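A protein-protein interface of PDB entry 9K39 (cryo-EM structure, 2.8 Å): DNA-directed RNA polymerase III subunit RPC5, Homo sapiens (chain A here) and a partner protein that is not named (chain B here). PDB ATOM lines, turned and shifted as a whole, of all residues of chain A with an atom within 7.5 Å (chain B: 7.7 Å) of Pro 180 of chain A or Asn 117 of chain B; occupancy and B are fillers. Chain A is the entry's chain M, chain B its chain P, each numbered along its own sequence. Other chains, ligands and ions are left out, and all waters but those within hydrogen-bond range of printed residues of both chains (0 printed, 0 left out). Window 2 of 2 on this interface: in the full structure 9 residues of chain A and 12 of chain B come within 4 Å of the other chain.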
ATOM      1  N   PHE A 177       5.794   7.746  16.026  1.00  0.00           N
ATOM      2  CA  PHE A 177       5.074   8.745  15.251  1.00  0.00           C
ATOM      3  C   PHE A 177       4.110   9.515  16.140  1.00  0.00           C
ATOM      4  O   PHE A 177       3.324   8.922  16.885  1.00  0.00           O
ATOM      5  CB  PHE A 177       4.301   8.082  14.110  1.00  0.00           C
ATOM      6  CG  PHE A 177       5.142   7.746  12.913  1.00  0.00           C
ATOM      7  CD1 PHE A 177       6.477   8.101  12.861  1.00  0.00           C
ATOM      8  CD2 PHE A 177       4.586   7.088  11.829  1.00  0.00           C
ATOM      9  CE1 PHE A 177       7.243   7.792  11.758  1.00  0.00           C
ATOM     10  CE2 PHE A 177       5.344   6.781  10.719  1.00  0.00           C
ATOM     11  CZ  PHE A 177       6.674   7.136  10.681  1.00  0.00           C
ATOM     12  N   SER A 178       4.169  10.845  16.063  1.00  0.00           N
ATOM     13  CA  SER A 178       3.147  11.690  16.674  1.00  0.00           C
ATOM     14  C   SER A 178       1.920  11.626  15.770  1.00  0.00           C
ATOM     15  O   SER A 178       1.609  12.550  15.012  1.00  0.00           O
ATOM     16  CB  SER A 178       3.651  13.118  16.855  1.00  0.00           C
ATOM     17  OG  SER A 178       3.955  13.716  15.608  1.00  0.00           O
ATOM     18  N   ARG A 179       1.225  10.496  15.843  1.00  0.00           N
ATOM     19  CA  ARG A 179       0.107  10.228  14.950  1.00  0.00           C
ATOM     20  C   ARG A 179      -0.979  11.281  15.129  1.00  0.00           C
ATOM     21  O   ARG A 179      -1.274  11.673  16.268  1.00  0.00           O
ATOM     22  CB  ARG A 179      -0.475   8.839  15.217  1.00  0.00           C
ATOM     23  CG  ARG A 179       0.502   7.689  15.041  1.00  0.00           C
ATOM     24  CD  ARG A 179      -0.189   6.359  15.303  1.00  0.00           C
ATOM     25  NE  ARG A 179       0.717   5.223  15.167  1.00  0.00           N
ATOM     26  CZ  ARG A 179       0.355   3.956  15.342  1.00  0.00           C
ATOM     27  NH1 ARG A 179      -0.898   3.662  15.664  1.00  0.00           N
ATOM     28  NH2 ARG A 179       1.244   2.983  15.198  1.00  0.00           N
ATOM     29  N   PRO A 180      -1.581  11.777  14.047  1.00  0.00           N
ATOM     30  CA  PRO A 180      -2.734  12.671  14.203  1.00  0.00           C
ATOM     31  C   PRO A 180      -3.894  11.937  14.854  1.00  0.00           C
ATOM     32  O   PRO A 180      -4.501  11.048  14.249  1.00  0.00           O
ATOM     33  CB  PRO A 180      -3.054  13.094  12.765  1.00  0.00           C
ATOM     34  CG  PRO A 180      -2.489  12.003  11.916  1.00  0.00           C
ATOM     35  CD  PRO A 180      -1.259  11.525  12.633  1.00  0.00           C
ATOM     36  N   GLU A 181      -4.206  12.303  16.093  1.00  0.00           N
ATOM     37  CA  GLU A 181      -5.196  11.564  16.860  1.00  0.00           C
ATOM     38  C   GLU A 181      -6.603  11.929  16.410  1.00  0.00           C
ATOM     39  O   GLU A 181      -6.922  13.103  16.200  1.00  0.00           O
ATOM     40  CB  GLU A 181      -5.025  11.848  18.352  1.00  0.00           C
ATOM     41  CG  GLU A 181      -5.802  10.907  19.255  1.00  0.00           C
ATOM     42  CD  GLU A 181      -5.586  11.205  20.726  1.00  0.00           C
ATOM     43  OE1 GLU A 181      -5.099  12.311  21.045  1.00  0.00           O
ATOM     44  OE2 GLU A 181      -5.900  10.336  21.565  1.00  0.00           O
ATOM     45  N   SER A 182      -7.445  10.909  16.251  1.00  0.00           N
ATOM     46  CA  SER A 182      -8.841  11.141  15.918  1.00  0.00           C
ATOM     47  C   SER A 182      -9.510  11.958  17.015  1.00  0.00           C
ATOM     48  O   SER A 182      -9.156  11.851  18.193  1.00  0.00           O
ATOM     49  CB  SER A 182      -9.572   9.813  15.719  1.00  0.00           C
ATOM     50  OG  SER A 182      -9.504   9.012  16.886  1.00  0.00           O
ATOM     51  N   GLU A 183     -10.478  12.790  16.618  1.00  0.00           N
ATOM     52  CA  GLU A 183     -11.118  13.689  17.574  1.00  0.00           C
ATOM     53  C   GLU A 183     -11.787  12.923  18.707  1.00  0.00           C
ATOM     54  O   GLU A 183     -11.794  13.392  19.851  1.00  0.00           O
ATOM     55  CB  GLU A 183     -12.129  14.580  16.852  1.00  0.00           C
ATOM     56  CG  GLU A 183     -12.611  15.764  17.674  1.00  0.00           C
ATOM     57  CD  GLU A 183     -13.349  16.789  16.837  1.00  0.00           C
ATOM     58  OE1 GLU A 183     -13.574  16.529  15.635  1.00  0.00           O
ATOM     59  OE2 GLU A 183     -13.701  17.859  17.378  1.00  0.00           O
ATOM     60  N   ALA A 185     -10.738   9.957  19.942  1.00  0.00           N
ATOM     61  CA  ALA A 185      -9.660   9.506  20.819  1.00  0.00           C
ATOM     62  C   ALA A 185      -9.034  10.677  21.566  1.00  0.00           C
ATOM     63  O   ALA A 185      -8.620  10.532  22.722  1.00  0.00           O
ATOM     64  CB  ALA A 185      -8.606   8.752  20.012  1.00  0.00           C
ATOM     65  N   GLN B  91       5.271  16.216   7.453  1.00  0.00           N
ATOM     66  CA  GLN B  91       4.837  14.887   7.029  1.00  0.00           C
ATOM     67  C   GLN B  91       5.974  14.104   6.381  1.00  0.00           C
ATOM     68  O   GLN B  91       6.035  12.875   6.511  1.00  0.00           O
ATOM     69  CB  GLN B  91       3.652  14.999   6.066  1.00  0.00           C
ATOM     70  CG  GLN B  91       2.305  15.211   6.749  1.00  0.00           C
ATOM     71  CD  GLN B  91       2.214  16.531   7.490  1.00  0.00           C
ATOM     72  OE1 GLN B  91       2.928  17.485   7.180  1.00  0.00           O
ATOM     73  NE2 GLN B  91       1.333  16.592   8.483  1.00  0.00           N
ATOM     74  N   LEU B  94       7.716  12.772   9.259  1.00  0.00           N
ATOM     75  CA  LEU B  94       6.758  11.907   9.937  1.00  0.00           C
ATOM     76  C   LEU B  94       6.363  10.699   9.101  1.00  0.00           C
ATOM     77  O   LEU B  94       5.418   9.991   9.462  1.00  0.00           O
ATOM     78  CB  LEU B  94       5.512  12.713  10.312  1.00  0.00           C
ATOM     79  CG  LEU B  94       4.680  12.234  11.503  1.00  0.00           C
ATOM     80  CD1 LEU B  94       5.485  12.348  12.788  1.00  0.00           C
ATOM     81  CD2 LEU B  94       3.382  13.018  11.602  1.00  0.00           C
ATOM     82  N   ARG B 110       0.750  -0.742   3.102  1.00  0.00           N
ATOM     83  CA  ARG B 110      -0.384  -0.826   4.018  1.00  0.00           C
ATOM     84  C   ARG B 110       0.042  -0.520   5.450  1.00  0.00           C
ATOM     85  O   ARG B 110      -0.641   0.221   6.166  1.00  0.00           O
ATOM     86  CB  ARG B 110      -1.026  -2.208   3.936  1.00  0.00           C
ATOM     87  CG  ARG B 110      -2.218  -2.392   4.858  1.00  0.00           C
ATOM     88  CD  ARG B 110      -2.451  -3.861   5.181  1.00  0.00           C
ATOM     89  NE  ARG B 110      -2.681  -4.662   3.983  1.00  0.00           N
ATOM     90  CZ  ARG B 110      -3.886  -4.962   3.503  1.00  0.00           C
ATOM     91  NH1 ARG B 110      -4.977  -4.523   4.120  1.00  0.00           N
ATOM     92  NH2 ARG B 110      -4.000  -5.698   2.407  1.00  0.00           N
ATOM     93  N   ASP B 111       1.170  -1.087   5.883  1.00  0.00           N
ATOM     94  CA  ASP B 111       1.641  -0.843   7.242  1.00  0.00           C
ATOM     95  C   ASP B 111       2.098   0.602   7.415  1.00  0.00           C
ATOM     96  O   ASP B 111       1.908   1.193   8.484  1.00  0.00           O
ATOM     97  CB  ASP B 111       2.766  -1.813   7.590  1.00  0.00           C
ATOM     98  CG  ASP B 111       2.347  -3.262   7.447  1.00  0.00           C
ATOM     99  OD1 ASP B 111       1.147  -3.557   7.634  1.00  0.00           O
ATOM    100  OD2 ASP B 111       3.215  -4.106   7.144  1.00  0.00           O
ATOM    101  N   ILE B 112       2.704   1.185   6.377  1.00  0.00           N
ATOM    102  CA  ILE B 112       3.080   2.595   6.439  1.00  0.00           C
ATOM    103  C   ILE B 112       1.840   3.466   6.591  1.00  0.00           C
ATOM    104  O   ILE B 112       1.814   4.404   7.396  1.00  0.00           O
ATOM    105  CB  ILE B 112       3.899   2.990   5.197  1.00  0.00           C
ATOM    106  CG1 ILE B 112       5.190   2.174   5.117  1.00  0.00           C
ATOM    107  CG2 ILE B 112       4.225   4.474   5.225  1.00  0.00           C
ATOM    108  CD1 ILE B 112       6.040   2.495   3.907  1.00  0.00           C
ATOM    109  N   ARG B 113       0.790   3.163   5.825  1.00  0.00           N
ATOM    110  CA  ARG B 113      -0.458   3.914   5.936  1.00  0.00           C
ATOM    111  C   ARG B 113      -1.079   3.755   7.319  1.00  0.00           C
ATOM    112  O   ARG B 113      -1.587   4.725   7.896  1.00  0.00           O
ATOM    113  CB  ARG B 113      -1.437   3.457   4.854  1.00  0.00           C
ATOM    114  CG  ARG B 113      -2.859   3.952   5.046  1.00  0.00           C
ATOM    115  CD  ARG B 113      -3.802   3.312   4.041  1.00  0.00           C
ATOM    116  NE  ARG B 113      -5.196   3.677   4.287  1.00  0.00           N
ATOM    117  CZ  ARG B 113      -6.221   3.221   3.576  1.00  0.00           C
ATOM    118  NH1 ARG B 113      -6.014   2.380   2.573  1.00  0.00           N
ATOM    119  NH2 ARG B 113      -7.457   3.606   3.870  1.00  0.00           N
ATOM    120  N   TYR B 114      -1.044   2.539   7.870  1.00  0.00           N
ATOM    121  CA  TYR B 114      -1.663   2.300   9.172  1.00  0.00           C
ATOM    122  C   TYR B 114      -0.881   2.974  10.296  1.00  0.00           C
ATOM    123  O   TYR B 114      -1.481   3.482  11.252  1.00  0.00           O
ATOM    124  CB  TYR B 114      -1.789   0.798   9.426  1.00  0.00           C
ATOM    125  CG  TYR B 114      -2.947   0.151   8.704  1.00  0.00           C
ATOM    126  CD1 TYR B 114      -4.011   0.913   8.234  1.00  0.00           C
ATOM    127  CD2 TYR B 114      -2.981  -1.221   8.489  1.00  0.00           C
ATOM    128  CE1 TYR B 114      -5.074   0.326   7.573  1.00  0.00           C
ATOM    129  CE2 TYR B 114      -4.040  -1.816   7.831  1.00  0.00           C
ATOM    130  CZ  TYR B 114      -5.083  -1.037   7.374  1.00  0.00           C
ATOM    131  OH  TYR B 114      -6.139  -1.626   6.715  1.00  0.00           O
ATOM    132  N   LYS B 115       0.448   2.993  10.203  1.00  0.00           N
ATOM    133  CA  LYS B 115       1.248   3.646  11.234  1.00  0.00           C
ATOM    134  C   LYS B 115       1.214   5.160  11.097  1.00  0.00           C
ATOM    135  O   LYS B 115       1.376   5.875  12.092  1.00  0.00           O
ATOM    136  CB  LYS B 115       2.692   3.143  11.189  1.00  0.00           C
ATOM    137  CG  LYS B 115       2.888   1.723  11.704  1.00  0.00           C
ATOM    138  CD  LYS B 115       4.362   1.347  11.703  1.00  0.00           C
ATOM    139  CE  LYS B 115       4.584  -0.078  12.185  1.00  0.00           C
ATOM    140  NZ  LYS B 115       4.017  -1.083  11.242  1.00  0.00           N
ATOM    141  N   SER B 116       1.002   5.672   9.884  1.00  0.00           N
ATOM    142  CA  SER B 116       0.940   7.107   9.662  1.00  0.00           C
ATOM    143  C   SER B 116      -0.448   7.691   9.884  1.00  0.00           C
ATOM    144  O   SER B 116      -0.570   8.914  10.016  1.00  0.00           O
ATOM    145  CB  SER B 116       1.412   7.439   8.242  1.00  0.00           C
ATOM    146  OG  SER B 116       0.589   6.814   7.273  1.00  0.00           O
ATOM    147  N   ASN B 117      -1.486   6.850   9.934  1.00  0.00           N
ATOM    148  CA  ASN B 117      -2.866   7.295  10.135  1.00  0.00           C
ATOM    149  C   ASN B 117      -3.259   8.357   9.109  1.00  0.00           C
ATOM    150  O   ASN B 117      -3.926   9.346   9.427  1.00  0.00           O
ATOM    151  CB  ASN B 117      -3.086   7.805  11.564  1.00  0.00           C
ATOM    152  CG  ASN B 117      -4.539   7.729  11.996  1.00  0.00           C
ATOM    153  OD1 ASN B 117      -5.451   7.774  11.169  1.00  0.00           O
ATOM    154  ND2 ASN B 117      -4.763   7.608  13.300  1.00  0.00           N
ATOM    155  N   LEU B 118      -2.840   8.153   7.869  1.00  0.00           N
ATOM    156  CA  LEU B 118      -3.113   9.053   6.762  1.00  0.00           C
ATOM    157  C   LEU B 118      -3.797   8.284   5.645  1.00  0.00           C
ATOM    158  O   LEU B 118      -3.625   7.066   5.525  1.00  0.00           O
ATOM    159  CB  LEU B 118      -1.820   9.695   6.237  1.00  0.00           C
ATOM    160  CG  LEU B 118      -1.151  10.731   7.141  1.00  0.00           C
ATOM    161  CD1 LEU B 118       0.188  11.158   6.560  1.00  0.00           C
ATOM    162  CD2 LEU B 118      -2.061  11.933   7.332  1.00  0.00           C
ATOM    163  N   PRO B 119      -4.588   8.962   4.818  1.00  0.00           N
ATOM    164  CA  PRO B 119      -5.223   8.286   3.681  1.00  0.00           C
ATOM    165  C   PRO B 119      -4.185   7.795   2.679  1.00  0.00           C
ATOM    166  O   PRO B 119      -2.999   8.120   2.747  1.00  0.00           O
ATOM    167  CB  PRO B 119      -6.124   9.366   3.076  1.00  0.00           C
ATOM    168  CG  PRO B 119      -6.347  10.340   4.189  1.00  0.00           C
ATOM    169  CD  PRO B 119      -5.071  10.344   4.975  1.00  0.00           C
ATOM    170  N   LEU B 120      -4.662   6.990   1.729  1.00  0.00           N
ATOM    171  CA  LEU B 120      -3.756   6.342   0.785  1.00  0.00           C
ATOM    172  C   LEU B 120      -3.145   7.346  -0.186  1.00  0.00           C
ATOM    173  O   LEU B 120      -1.989   7.196  -0.597  1.00  0.00           O
ATOM    174  CB  LEU B 120      -4.497   5.240   0.028  1.00  0.00           C
ATOM    175  CG  LEU B 120      -3.652   4.342  -0.877  1.00  0.00           C
ATOM    176  CD1 LEU B 120      -2.561   3.648  -0.076  1.00  0.00           C
ATOM    177  CD2 LEU B 120      -4.531   3.327  -1.583  1.00  0.00           C
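The backbone carbonyl oxygen (O) of Lys 115 of chain B lies within hydrogen-bond range of the guanidinium group (NE) of Arg 179 of chain A (3.2 Å).
The side-chain hydroxyl (OG) of Ser 116 of chain B is in hydrogen-bond range of the backbone carbonyl oxygen (O) of Ile 112 of chain B (2.7 Å). OG of Ser 116 of chain B lies within hydrogen-bond range of O of Arg 113 of chain B (3.1 Å).
Among the printed residues, pairs that only touch across the chains: Phe 177 of chain A with Leu 94 of chain B, Phe 177 of chain A with Lys 115 of chain B, Ser 178 of chain A with Leu 94 of chain B, Pro 180 of chain A with Ser 116 of chain B and Pro 180 of chain A with Asn 117 of chain B.
Of the printed residues of chain B, Phe 177 of chain A touches Leu 94 and Lys 115. Printed residues of chain B within 4 Å of Ser 178 of chain A: Leu 94 (3.5 Å). Of the printed residues of chain B, Arg 179 of chain A touches Lys 115. Of chain B, only Ser 116 and Asn 117 come within 4 Å of Pro 180 of chain A. Of the printed residues of chain A, Leu 94 of chain B touches Phe 177 and Ser 178. Arg 110 of chain B touches none of the printed residues of chain A. Ile 112 of chain B touches none of the printed residues of chain A. Of the printed residues of chain A, Lys 115 of chain B touches Phe 177 and Arg 179. Printed residues of chain A within 4 Å of Ser 116 of chain B: Pro 180. Printed residues of chain A within 4 Å of Asn 117 of chain B: Pro 180. The nearest residue of chain B that does not touch Pro 180 of chain A is Leu 118 of chain B (4.6 Å). The nearest residue of chain A that does not touch Asn 117 of chain B is Arg 179 of chain A (4.6 Å). The nearest printed residue of chain A that does not touch Lys 115 of chain B is Pro 180 of chain A (6.3 Å).
Printed residues of chain A that touch a printed residue of chain B: Phe 177, Ser 178, Arg 179 and Pro 180. Printed residues of chain B that touch a printed residue of chain A: Leu 94, Lys 115, Ser 116 and Asn 117. Hydrophobic or aromatic side chains of chain B within 4 Å of the printed part of chain A: Leu 94.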
